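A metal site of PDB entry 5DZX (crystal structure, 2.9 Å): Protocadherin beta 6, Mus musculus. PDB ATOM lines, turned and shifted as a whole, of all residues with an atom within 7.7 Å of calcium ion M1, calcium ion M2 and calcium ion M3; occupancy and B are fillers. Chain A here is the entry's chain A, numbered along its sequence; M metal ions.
The guanidinium group of Arg 64 lies close to the side-chain carboxylate of Glu 65 (3.3 Å).
A ring nitrogen (ND1) of His 101 lies close to the side-chain carboxylate (OD1) of Asp 100 (2.9 Å).
The side-chain amino group of Lys 194 is in hydrogen-bond range of the backbone carbonyl oxygen of Asn 99, at 3.2 Å.
The side-chain carboxylate (OD2) of Asp 97 is in salt-bridge range of the guanidinium group (NH2) of Arg 64, 3.8 Å away.
OD2 of Asp 97 is in hydrogen-bond range of N of Ile 134.
N of Asp 188 is in hydrogen-bond range of O of Lys 194 (3.3 Å).
The side-chain carboxylate of Asp 188 is in hydrogen-bond range of the backbone NH of Gly 190, at 2.9 Å.
The backbone carbonyl oxygen of Pro 62 is in hydrogen-bond range of the backbone NH of Glu 10 (2.7 Å).
Calcium ion M1 is bound by the side-chain carboxylate (OE2) of Glu 9 (2.2 Å), the side-chain carboxylate (OD2) of Asp 100 (2.3 Å), the side-chain carboxylate (OD1) of Asp 63 (2.5 Å), the side-chain carboxylate (OE2) of Glu 10 (2.6 Å) and the side-chain carboxylate (OE1) of Glu 65 (2.7 Å).
Calcium ion M1 has five donor atoms within binding distance.
Calcium ion M3 is bound by O of His 101 (2.3 Å), OD1 of Asn 99 (2.4 Å), O of Asn 137 (2.5 Å), OD2 of Asp 133 (2.6 Å), OD2 of Asp 188 (2.6 Å) and OD2 of Asp 131 (2.7 Å).
Slightly farther from calcium ion M3 lies the side-chain carboxylate (OD1) of Asp 131 (3.0 Å).
Calcium ion M2 is bound by the side-chain carboxylate (OE2) of Glu 65 (2.2 Å).
OE1 of Glu 9 binds calcium ion M2, 2.4 Å away.
OD1 of Asp 97 binds calcium ion M2 (2.4 Å).
Calcium ion M2 is bound by OD1 of Asp 100 (2.4 Å).
The side-chain carboxylate (OD1) of Asp 133 binds calcium ion M2, 2.5 Å away.
Calcium ion M2 is bound by O of Ile 98 (2.5 Å).
Six residues have an atom within 4 Å of calcium ion M2: Glu 9, Glu 65, Asp 97, Ile 98, Asp 100 and Asp 133.
Six residues have an atom within 4 Å of calcium ion M3: Asn 99, His 101, Asp 131, Asp 133, Asn 137 and Asp 188.
The nearest printed residue that does not touch calcium ion M3 is Ser 102 (4.5 Å).
Within 4 Å of calcium ion M1: Glu 9, Glu 10, Asp 63, Glu 65, Asp 100 and His 101.
Along chain A the residues within 4 Å of calcium ion M1 span positions 9 to 101.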
ATOM      1  N   GLU A   9     -20.713  15.103  -1.184  1.00  0.00           N
ATOM      2  CA  GLU A   9     -20.877  16.248  -0.303  1.00  0.00           C
ATOM      3  C   GLU A   9     -19.851  16.214   0.821  1.00  0.00           C
ATOM      4  O   GLU A   9     -19.379  15.143   1.213  1.00  0.00           O
ATOM      5  CB  GLU A   9     -22.299  16.270   0.259  1.00  0.00           C
ATOM      6  CG  GLU A   9     -22.599  17.417   1.201  1.00  0.00           C
ATOM      7  CD  GLU A   9     -23.676  17.072   2.197  1.00  0.00           C
ATOM      8  OE1 GLU A   9     -24.443  16.117   1.934  1.00  0.00           O
ATOM      9  OE2 GLU A   9     -23.763  17.743   3.244  1.00  0.00           O
ATOM     10  N   GLU A  10     -19.475  17.395   1.322  1.00  0.00           N
ATOM     11  CA  GLU A  10     -18.602  17.538   2.482  1.00  0.00           C
ATOM     12  C   GLU A  10     -17.215  16.926   2.261  1.00  0.00           C
ATOM     13  O   GLU A  10     -16.565  16.487   3.200  1.00  0.00           O
ATOM     14  CB  GLU A  10     -19.233  16.921   3.732  1.00  0.00           C
ATOM     15  CG  GLU A  10     -20.591  17.499   4.122  1.00  0.00           C
ATOM     16  CD  GLU A  10     -20.487  18.858   4.800  1.00  0.00           C
ATOM     17  OE1 GLU A  10     -19.373  19.410   4.897  1.00  0.00           O
ATOM     18  OE2 GLU A  10     -21.538  19.369   5.242  1.00  0.00           O
ATOM     19  N   PRO A  62     -17.934  21.541   0.370  1.00  0.00           N
ATOM     20  CA  PRO A  62     -19.289  21.724  -0.165  1.00  0.00           C
ATOM     21  C   PRO A  62     -20.365  21.072   0.699  1.00  0.00           C
ATOM     22  O   PRO A  62     -20.313  19.887   0.985  1.00  0.00           O
ATOM     23  CB  PRO A  62     -19.204  21.028  -1.528  1.00  0.00           C
ATOM     24  CG  PRO A  62     -18.196  19.949  -1.325  1.00  0.00           C
ATOM     25  CD  PRO A  62     -17.200  20.469  -0.317  1.00  0.00           C
ATOM     26  N   ASP A  63     -21.344  21.878   1.108  1.00  0.00           N
ATOM     27  CA  ASP A  63     -22.474  21.374   1.875  1.00  0.00           C
ATOM     28  C   ASP A  63     -23.731  21.369   1.018  1.00  0.00           C
ATOM     29  O   ASP A  63     -24.234  22.418   0.627  1.00  0.00           O
ATOM     30  CB  ASP A  63     -22.688  22.209   3.135  1.00  0.00           C
ATOM     31  CG  ASP A  63     -23.752  21.636   4.043  1.00  0.00           C
ATOM     32  OD1 ASP A  63     -23.937  20.402   4.031  1.00  0.00           O
ATOM     33  OD2 ASP A  63     -24.422  22.423   4.756  1.00  0.00           O
ATOM     34  N   ARG A  64     -24.230  20.166   0.720  1.00  0.00           N
ATOM     35  CA  ARG A  64     -25.387  19.996  -0.144  1.00  0.00           C
ATOM     36  C   ARG A  64     -26.614  20.711   0.420  1.00  0.00           C
ATOM     37  O   ARG A  64     -27.275  21.483  -0.287  1.00  0.00           O
ATOM     38  CB  ARG A  64     -25.685  18.500  -0.337  1.00  0.00           C
ATOM     39  CG  ARG A  64     -26.298  18.128  -1.686  1.00  0.00           C
ATOM     40  CD  ARG A  64     -27.744  18.600  -1.832  1.00  0.00           C
ATOM     41  NE  ARG A  64     -28.526  18.355  -0.618  1.00  0.00           N
ATOM     42  CZ  ARG A  64     -29.086  17.191  -0.326  1.00  0.00           C
ATOM     43  NH1 ARG A  64     -29.791  17.046   0.792  1.00  0.00           N
ATOM     44  NH2 ARG A  64     -28.956  16.158  -1.145  1.00  0.00           N
ATOM     45  N   GLU A  65     -26.904  20.469   1.688  1.00  0.00           N
ATOM     46  CA  GLU A  65     -28.112  20.982   2.327  1.00  0.00           C
ATOM     47  C   GLU A  65     -28.126  22.504   2.455  1.00  0.00           C
ATOM     48  O   GLU A  65     -29.157  23.102   2.748  1.00  0.00           O
ATOM     49  CB  GLU A  65     -28.287  20.353   3.709  1.00  0.00           C
ATOM     50  CG  GLU A  65     -28.551  18.846   3.704  1.00  0.00           C
ATOM     51  CD  GLU A  65     -27.292  18.023   3.521  1.00  0.00           C
ATOM     52  OE1 GLU A  65     -26.205  18.515   3.885  1.00  0.00           O
ATOM     53  OE2 GLU A  65     -27.394  16.892   3.011  1.00  0.00           O
ATOM     54  N   ALA A  66     -26.969  23.132   2.231  1.00  0.00           N
ATOM     55  CA  ALA A  66     -26.851  24.580   2.377  1.00  0.00           C
ATOM     56  C   ALA A  66     -26.673  25.277   1.039  1.00  0.00           C
ATOM     57  O   ALA A  66     -26.785  26.501   0.947  1.00  0.00           O
ATOM     58  CB  ALA A  66     -25.687  24.919   3.301  1.00  0.00           C
ATOM     59  N   THR A  96     -22.870  14.822  -4.872  1.00  0.00           N
ATOM     60  CA  THR A  96     -23.552  13.618  -4.418  1.00  0.00           C
ATOM     61  C   THR A  96     -23.874  13.724  -2.933  1.00  0.00           C
ATOM     62  O   THR A  96     -23.014  14.091  -2.127  1.00  0.00           O
ATOM     63  CB  THR A  96     -22.724  12.353  -4.677  1.00  0.00           C
ATOM     64  OG1 THR A  96     -22.420  12.245  -6.074  1.00  0.00           O
ATOM     65  CG2 THR A  96     -23.497  11.109  -4.250  1.00  0.00           C
ATOM     66  N   ASP A  97     -25.106  13.385  -2.571  1.00  0.00           N
ATOM     67  CA  ASP A  97     -25.549  13.459  -1.185  1.00  0.00           C
ATOM     68  C   ASP A  97     -24.970  12.325  -0.353  1.00  0.00           C
ATOM     69  O   ASP A  97     -25.061  11.154  -0.732  1.00  0.00           O
ATOM     70  CB  ASP A  97     -27.070  13.436  -1.103  1.00  0.00           C
ATOM     71  CG  ASP A  97     -27.570  13.544   0.320  1.00  0.00           C
ATOM     72  OD1 ASP A  97     -26.937  14.276   1.115  1.00  0.00           O
ATOM     73  OD2 ASP A  97     -28.568  12.877   0.659  1.00  0.00           O
ATOM     74  N   ILE A  98     -24.403  12.672   0.790  1.00  0.00           N
ATOM     75  CA  ILE A  98     -23.888  11.678   1.717  1.00  0.00           C
ATOM     76  C   ILE A  98     -24.667  11.745   3.039  1.00  0.00           C
ATOM     77  O   ILE A  98     -24.986  12.833   3.515  1.00  0.00           O
ATOM     78  CB  ILE A  98     -22.387  11.879   1.971  1.00  0.00           C
ATOM     79  CG1 ILE A  98     -22.078  13.344   2.284  1.00  0.00           C
ATOM     80  CG2 ILE A  98     -21.586  11.437   0.750  1.00  0.00           C
ATOM     81  CD1 ILE A  98     -21.825  13.625   3.747  1.00  0.00           C
ATOM     82  N   ASN A  99     -24.977  10.577   3.595  1.00  0.00           N
ATOM     83  CA  ASN A  99     -25.804  10.493   4.793  1.00  0.00           C
ATOM     84  C   ASN A  99     -25.082  11.019   6.034  1.00  0.00           C
ATOM     85  O   ASN A  99     -24.469  10.246   6.769  1.00  0.00           O
ATOM     86  CB  ASN A  99     -26.238   9.042   5.017  1.00  0.00           C
ATOM     87  CG  ASN A  99     -27.319   8.917   6.077  1.00  0.00           C
ATOM     88  OD1 ASN A  99     -28.062   9.855   6.328  1.00  0.00           O
ATOM     89  ND2 ASN A  99     -27.401   7.746   6.702  1.00  0.00           N
ATOM     90  N   ASP A 100     -25.188  12.316   6.277  1.00  0.00           N
ATOM     91  CA  ASP A 100     -24.521  12.937   7.406  1.00  0.00           C
ATOM     92  C   ASP A 100     -25.511  13.591   8.360  1.00  0.00           C
ATOM     93  O   ASP A 100     -25.151  14.463   9.150  1.00  0.00           O
ATOM     94  CB  ASP A 100     -23.487  13.972   6.913  1.00  0.00           C
ATOM     95  CG  ASP A 100     -24.104  15.046   6.036  1.00  0.00           C
ATOM     96  OD1 ASP A 100     -25.215  14.835   5.496  1.00  0.00           O
ATOM     97  OD2 ASP A 100     -23.469  16.108   5.859  1.00  0.00           O
ATOM     98  N   HIS A 101     -26.762  13.152   8.295  1.00  0.00           N
ATOM     99  CA  HIS A 101     -27.800  13.640   9.194  1.00  0.00           C
ATOM    100  C   HIS A 101     -28.643  12.507   9.755  1.00  0.00           C
ATOM    101  O   HIS A 101     -29.111  11.643   9.012  1.00  0.00           O
ATOM    102  CB  HIS A 101     -28.699  14.655   8.471  1.00  0.00           C
ATOM    103  CG  HIS A 101     -28.046  15.980   8.247  1.00  0.00           C
ATOM    104  ND1 HIS A 101     -26.975  16.151   7.394  1.00  0.00           N
ATOM    105  CD2 HIS A 101     -28.314  17.197   8.776  1.00  0.00           C
ATOM    106  CE1 HIS A 101     -26.616  17.419   7.407  1.00  0.00           C
ATOM    107  NE2 HIS A 101     -27.406  18.077   8.231  1.00  0.00           N
ATOM    108  N   SER A 102     -28.850  12.511  11.067  1.00  0.00           N
ATOM    109  CA  SER A 102     -29.645  11.486  11.710  1.00  0.00           C
ATOM    110  C   SER A 102     -31.115  11.901  11.790  1.00  0.00           C
ATOM    111  O   SER A 102     -31.414  13.057  12.076  1.00  0.00           O
ATOM    112  CB  SER A 102     -29.113  11.182  13.110  1.00  0.00           C
ATOM    113  OG  SER A 102     -27.746  10.795  13.048  1.00  0.00           O
ATOM    114  N   PRO A 103     -32.029  10.946  11.543  1.00  0.00           N
ATOM    115  CA  PRO A 103     -33.462  11.209  11.681  1.00  0.00           C
ATOM    116  C   PRO A 103     -33.773  11.743  13.071  1.00  0.00           C
ATOM    117  O   PRO A 103     -33.320  11.192  14.066  1.00  0.00           O
ATOM    118  CB  PRO A 103     -34.095   9.834  11.471  1.00  0.00           C
ATOM    119  CG  PRO A 103     -33.121   9.108  10.613  1.00  0.00           C
ATOM    120  CD  PRO A 103     -31.767   9.571  11.088  1.00  0.00           C
ATOM    121  N   GLN A 130     -37.875  14.660  10.932  1.00  0.00           N
ATOM    122  CA  GLN A 130     -37.241  15.540   9.968  1.00  0.00           C
ATOM    123  C   GLN A 130     -35.815  15.089   9.646  1.00  0.00           C
ATOM    124  O   GLN A 130     -35.031  14.778  10.537  1.00  0.00           O
ATOM    125  CB  GLN A 130     -37.256  16.985  10.476  1.00  0.00           C
ATOM    126  CG  GLN A 130     -36.863  17.143  11.936  1.00  0.00           C
ATOM    127  CD  GLN A 130     -37.337  18.454  12.520  1.00  0.00           C
ATOM    128  OE1 GLN A 130     -38.078  19.198  11.884  1.00  0.00           O
ATOM    129  NE2 GLN A 130     -36.922  18.745  13.753  1.00  0.00           N
ATOM    130  N   ASP A 131     -35.499  15.070   8.363  1.00  0.00           N
ATOM    131  CA  ASP A 131     -34.168  14.699   7.892  1.00  0.00           C
ATOM    132  C   ASP A 131     -33.722  15.647   6.782  1.00  0.00           C
ATOM    133  O   ASP A 131     -34.473  15.899   5.844  1.00  0.00           O
ATOM    134  CB  ASP A 131     -34.153  13.245   7.395  1.00  0.00           C
ATOM    135  CG  ASP A 131     -32.760  12.659   7.338  1.00  0.00           C
ATOM    136  OD1 ASP A 131     -31.805  13.418   7.055  1.00  0.00           O
ATOM    137  OD2 ASP A 131     -32.610  11.447   7.571  1.00  0.00           O
ATOM    138  N   SER A 132     -32.509  16.165   6.902  1.00  0.00           N
ATOM    139  CA  SER A 132     -31.973  17.096   5.910  1.00  0.00           C
ATOM    140  C   SER A 132     -31.581  16.377   4.625  1.00  0.00           C
ATOM    141  O   SER A 132     -31.693  16.939   3.542  1.00  0.00           O
ATOM    142  CB  SER A 132     -30.763  17.843   6.477  1.00  0.00           C
ATOM    143  OG  SER A 132     -31.131  18.661   7.578  1.00  0.00           O
ATOM    144  N   ASP A 133     -31.138  15.131   4.756  1.00  0.00           N
ATOM    145  CA  ASP A 133     -30.731  14.336   3.600  1.00  0.00           C
ATOM    146  C   ASP A 133     -31.920  13.981   2.718  1.00  0.00           C
ATOM    147  O   ASP A 133     -33.075  14.184   3.104  1.00  0.00           O
ATOM    148  CB  ASP A 133     -30.019  13.057   4.061  1.00  0.00           C
ATOM    149  CG  ASP A 133     -28.772  13.344   4.870  1.00  0.00           C
ATOM    150  OD1 ASP A 133     -28.089  14.352   4.586  1.00  0.00           O
ATOM    151  OD2 ASP A 133     -28.475  12.555   5.794  1.00  0.00           O
ATOM    152  N   ILE A 134     -31.636  13.461   1.530  1.00  0.00           N
ATOM    153  CA  ILE A 134     -32.690  13.088   0.593  1.00  0.00           C
ATOM    154  C   ILE A 134     -32.441  11.693   0.034  1.00  0.00           C
ATOM    155  O   ILE A 134     -31.403  11.086   0.279  1.00  0.00           O
ATOM    156  CB  ILE A 134     -32.815  14.105  -0.565  1.00  0.00           C
ATOM    157  CG1 ILE A 134     -31.488  14.230  -1.331  1.00  0.00           C
ATOM    158  CG2 ILE A 134     -33.250  15.465  -0.052  1.00  0.00           C
ATOM    159  CD1 ILE A 134     -31.424  13.447  -2.625  1.00  0.00           C
ATOM    160  N   SER A 136     -32.124   7.919  -0.660  1.00  0.00           N
ATOM    161  CA  SER A 136     -31.847   6.753   0.178  1.00  0.00           C
ATOM    162  C   SER A 136     -31.286   7.162   1.540  1.00  0.00           C
ATOM    163  O   SER A 136     -31.335   6.382   2.495  1.00  0.00           O
ATOM    164  CB  SER A 136     -30.869   5.812  -0.534  1.00  0.00           C
ATOM    165  OG  SER A 136     -30.549   4.693   0.267  1.00  0.00           O
ATOM    166  N   ASN A 137     -30.746   8.365   1.630  1.00  0.00           N
ATOM    167  CA  ASN A 137     -30.155   8.862   2.871  1.00  0.00           C
ATOM    168  C   ASN A 137     -31.177   9.520   3.794  1.00  0.00           C
ATOM    169  O   ASN A 137     -30.836   9.929   4.906  1.00  0.00           O
ATOM    170  CB  ASN A 137     -29.027   9.836   2.569  1.00  0.00           C
ATOM    171  CG  ASN A 137     -27.816   9.157   1.962  1.00  0.00           C
ATOM    172  OD1 ASN A 137     -27.567   7.972   2.221  1.00  0.00           O
ATOM    173  ND2 ASN A 137     -27.057   9.884   1.151  1.00  0.00           N
ATOM    174  N   ALA A 138     -32.410   9.628   3.329  1.00  0.00           N
ATOM    175  CA  ALA A 138     -33.481  10.171   4.147  1.00  0.00           C
ATOM    176  C   ALA A 138     -34.162   9.052   4.936  1.00  0.00           C
ATOM    177  O   ALA A 138     -33.779   7.894   4.834  1.00  0.00           O
ATOM    178  CB  ALA A 138     -34.496  10.911   3.295  1.00  0.00           C
ATOM    179  N   VAL A 139     -35.175   9.416   5.711  1.00  0.00           N
ATOM    180  CA  VAL A 139     -35.962   8.447   6.460  1.00  0.00           C
ATOM    181  C   VAL A 139     -36.601   7.456   5.490  1.00  0.00           C
ATOM    182  O   VAL A 139     -37.168   7.862   4.476  1.00  0.00           O
ATOM    183  CB  VAL A 139     -37.039   9.133   7.309  1.00  0.00           C
ATOM    184  CG1 VAL A 139     -37.885   8.102   8.021  1.00  0.00           C
ATOM    185  CG2 VAL A 139     -36.394  10.078   8.305  1.00  0.00           C
ATOM    186  N   ASP A 188     -33.311   5.200   9.030  1.00  0.00           N
ATOM    187  CA  ASP A 188     -32.731   5.750   7.828  1.00  0.00           C
ATOM    188  C   ASP A 188     -32.464   4.634   6.822  1.00  0.00           C
ATOM    189  O   ASP A 188     -32.316   3.470   7.191  1.00  0.00           O
ATOM    190  CB  ASP A 188     -31.439   6.495   8.166  1.00  0.00           C
ATOM    191  CG  ASP A 188     -31.028   7.476   7.102  1.00  0.00           C
ATOM    192  OD1 ASP A 188     -30.386   7.048   6.113  1.00  0.00           O
ATOM    193  OD2 ASP A 188     -31.331   8.675   7.250  1.00  0.00           O
ATOM    194  N   GLY A 189     -32.401   4.991   5.537  1.00  0.00           N
ATOM    195  CA  GLY A 189     -32.169   4.010   4.494  1.00  0.00           C
ATOM    196  C   GLY A 189     -30.703   3.739   4.212  1.00  0.00           C
ATOM    197  O   GLY A 189     -30.356   2.740   3.581  1.00  0.00           O
ATOM    198  N   GLY A 190     -29.840   4.632   4.683  1.00  0.00           N
ATOM    199  CA  GLY A 190     -28.412   4.517   4.453  1.00  0.00           C
ATOM    200  C   GLY A 190     -27.776   3.322   5.136  1.00  0.00           C
ATOM    201  O   GLY A 190     -28.399   2.655   5.970  1.00  0.00           O
ATOM    202  N   LYS A 194     -29.380   5.198  10.468  1.00  0.00           N
ATOM    203  CA  LYS A 194     -29.321   6.048  11.666  1.00  0.00           C
ATOM    204  C   LYS A 194     -30.682   6.118  12.352  1.00  0.00           C
ATOM    205  O   LYS A 194     -31.725   6.192  11.691  1.00  0.00           O
ATOM    206  CB  LYS A 194     -28.826   7.454  11.306  1.00  0.00           C
ATOM    207  CG  LYS A 194     -27.393   7.476  10.815  1.00  0.00           C
ATOM    208  CD  LYS A 194     -26.904   8.888  10.530  1.00  0.00           C
ATOM    209  CE  LYS A 194     -25.432   8.886  10.145  1.00  0.00           C
ATOM    210  NZ  LYS A 194     -24.897  10.250   9.929  1.00  0.00           N
HETATM  211 CA    CA M   1     -23.955  18.306   5.314  1.00  0.00          CA
HETATM  212 CA    CA M   2     -26.151  15.072   3.263  1.00  0.00          CA
HETATM  213 CA    CA M   3     -30.052  10.951   7.060  1.00  0.00          CA
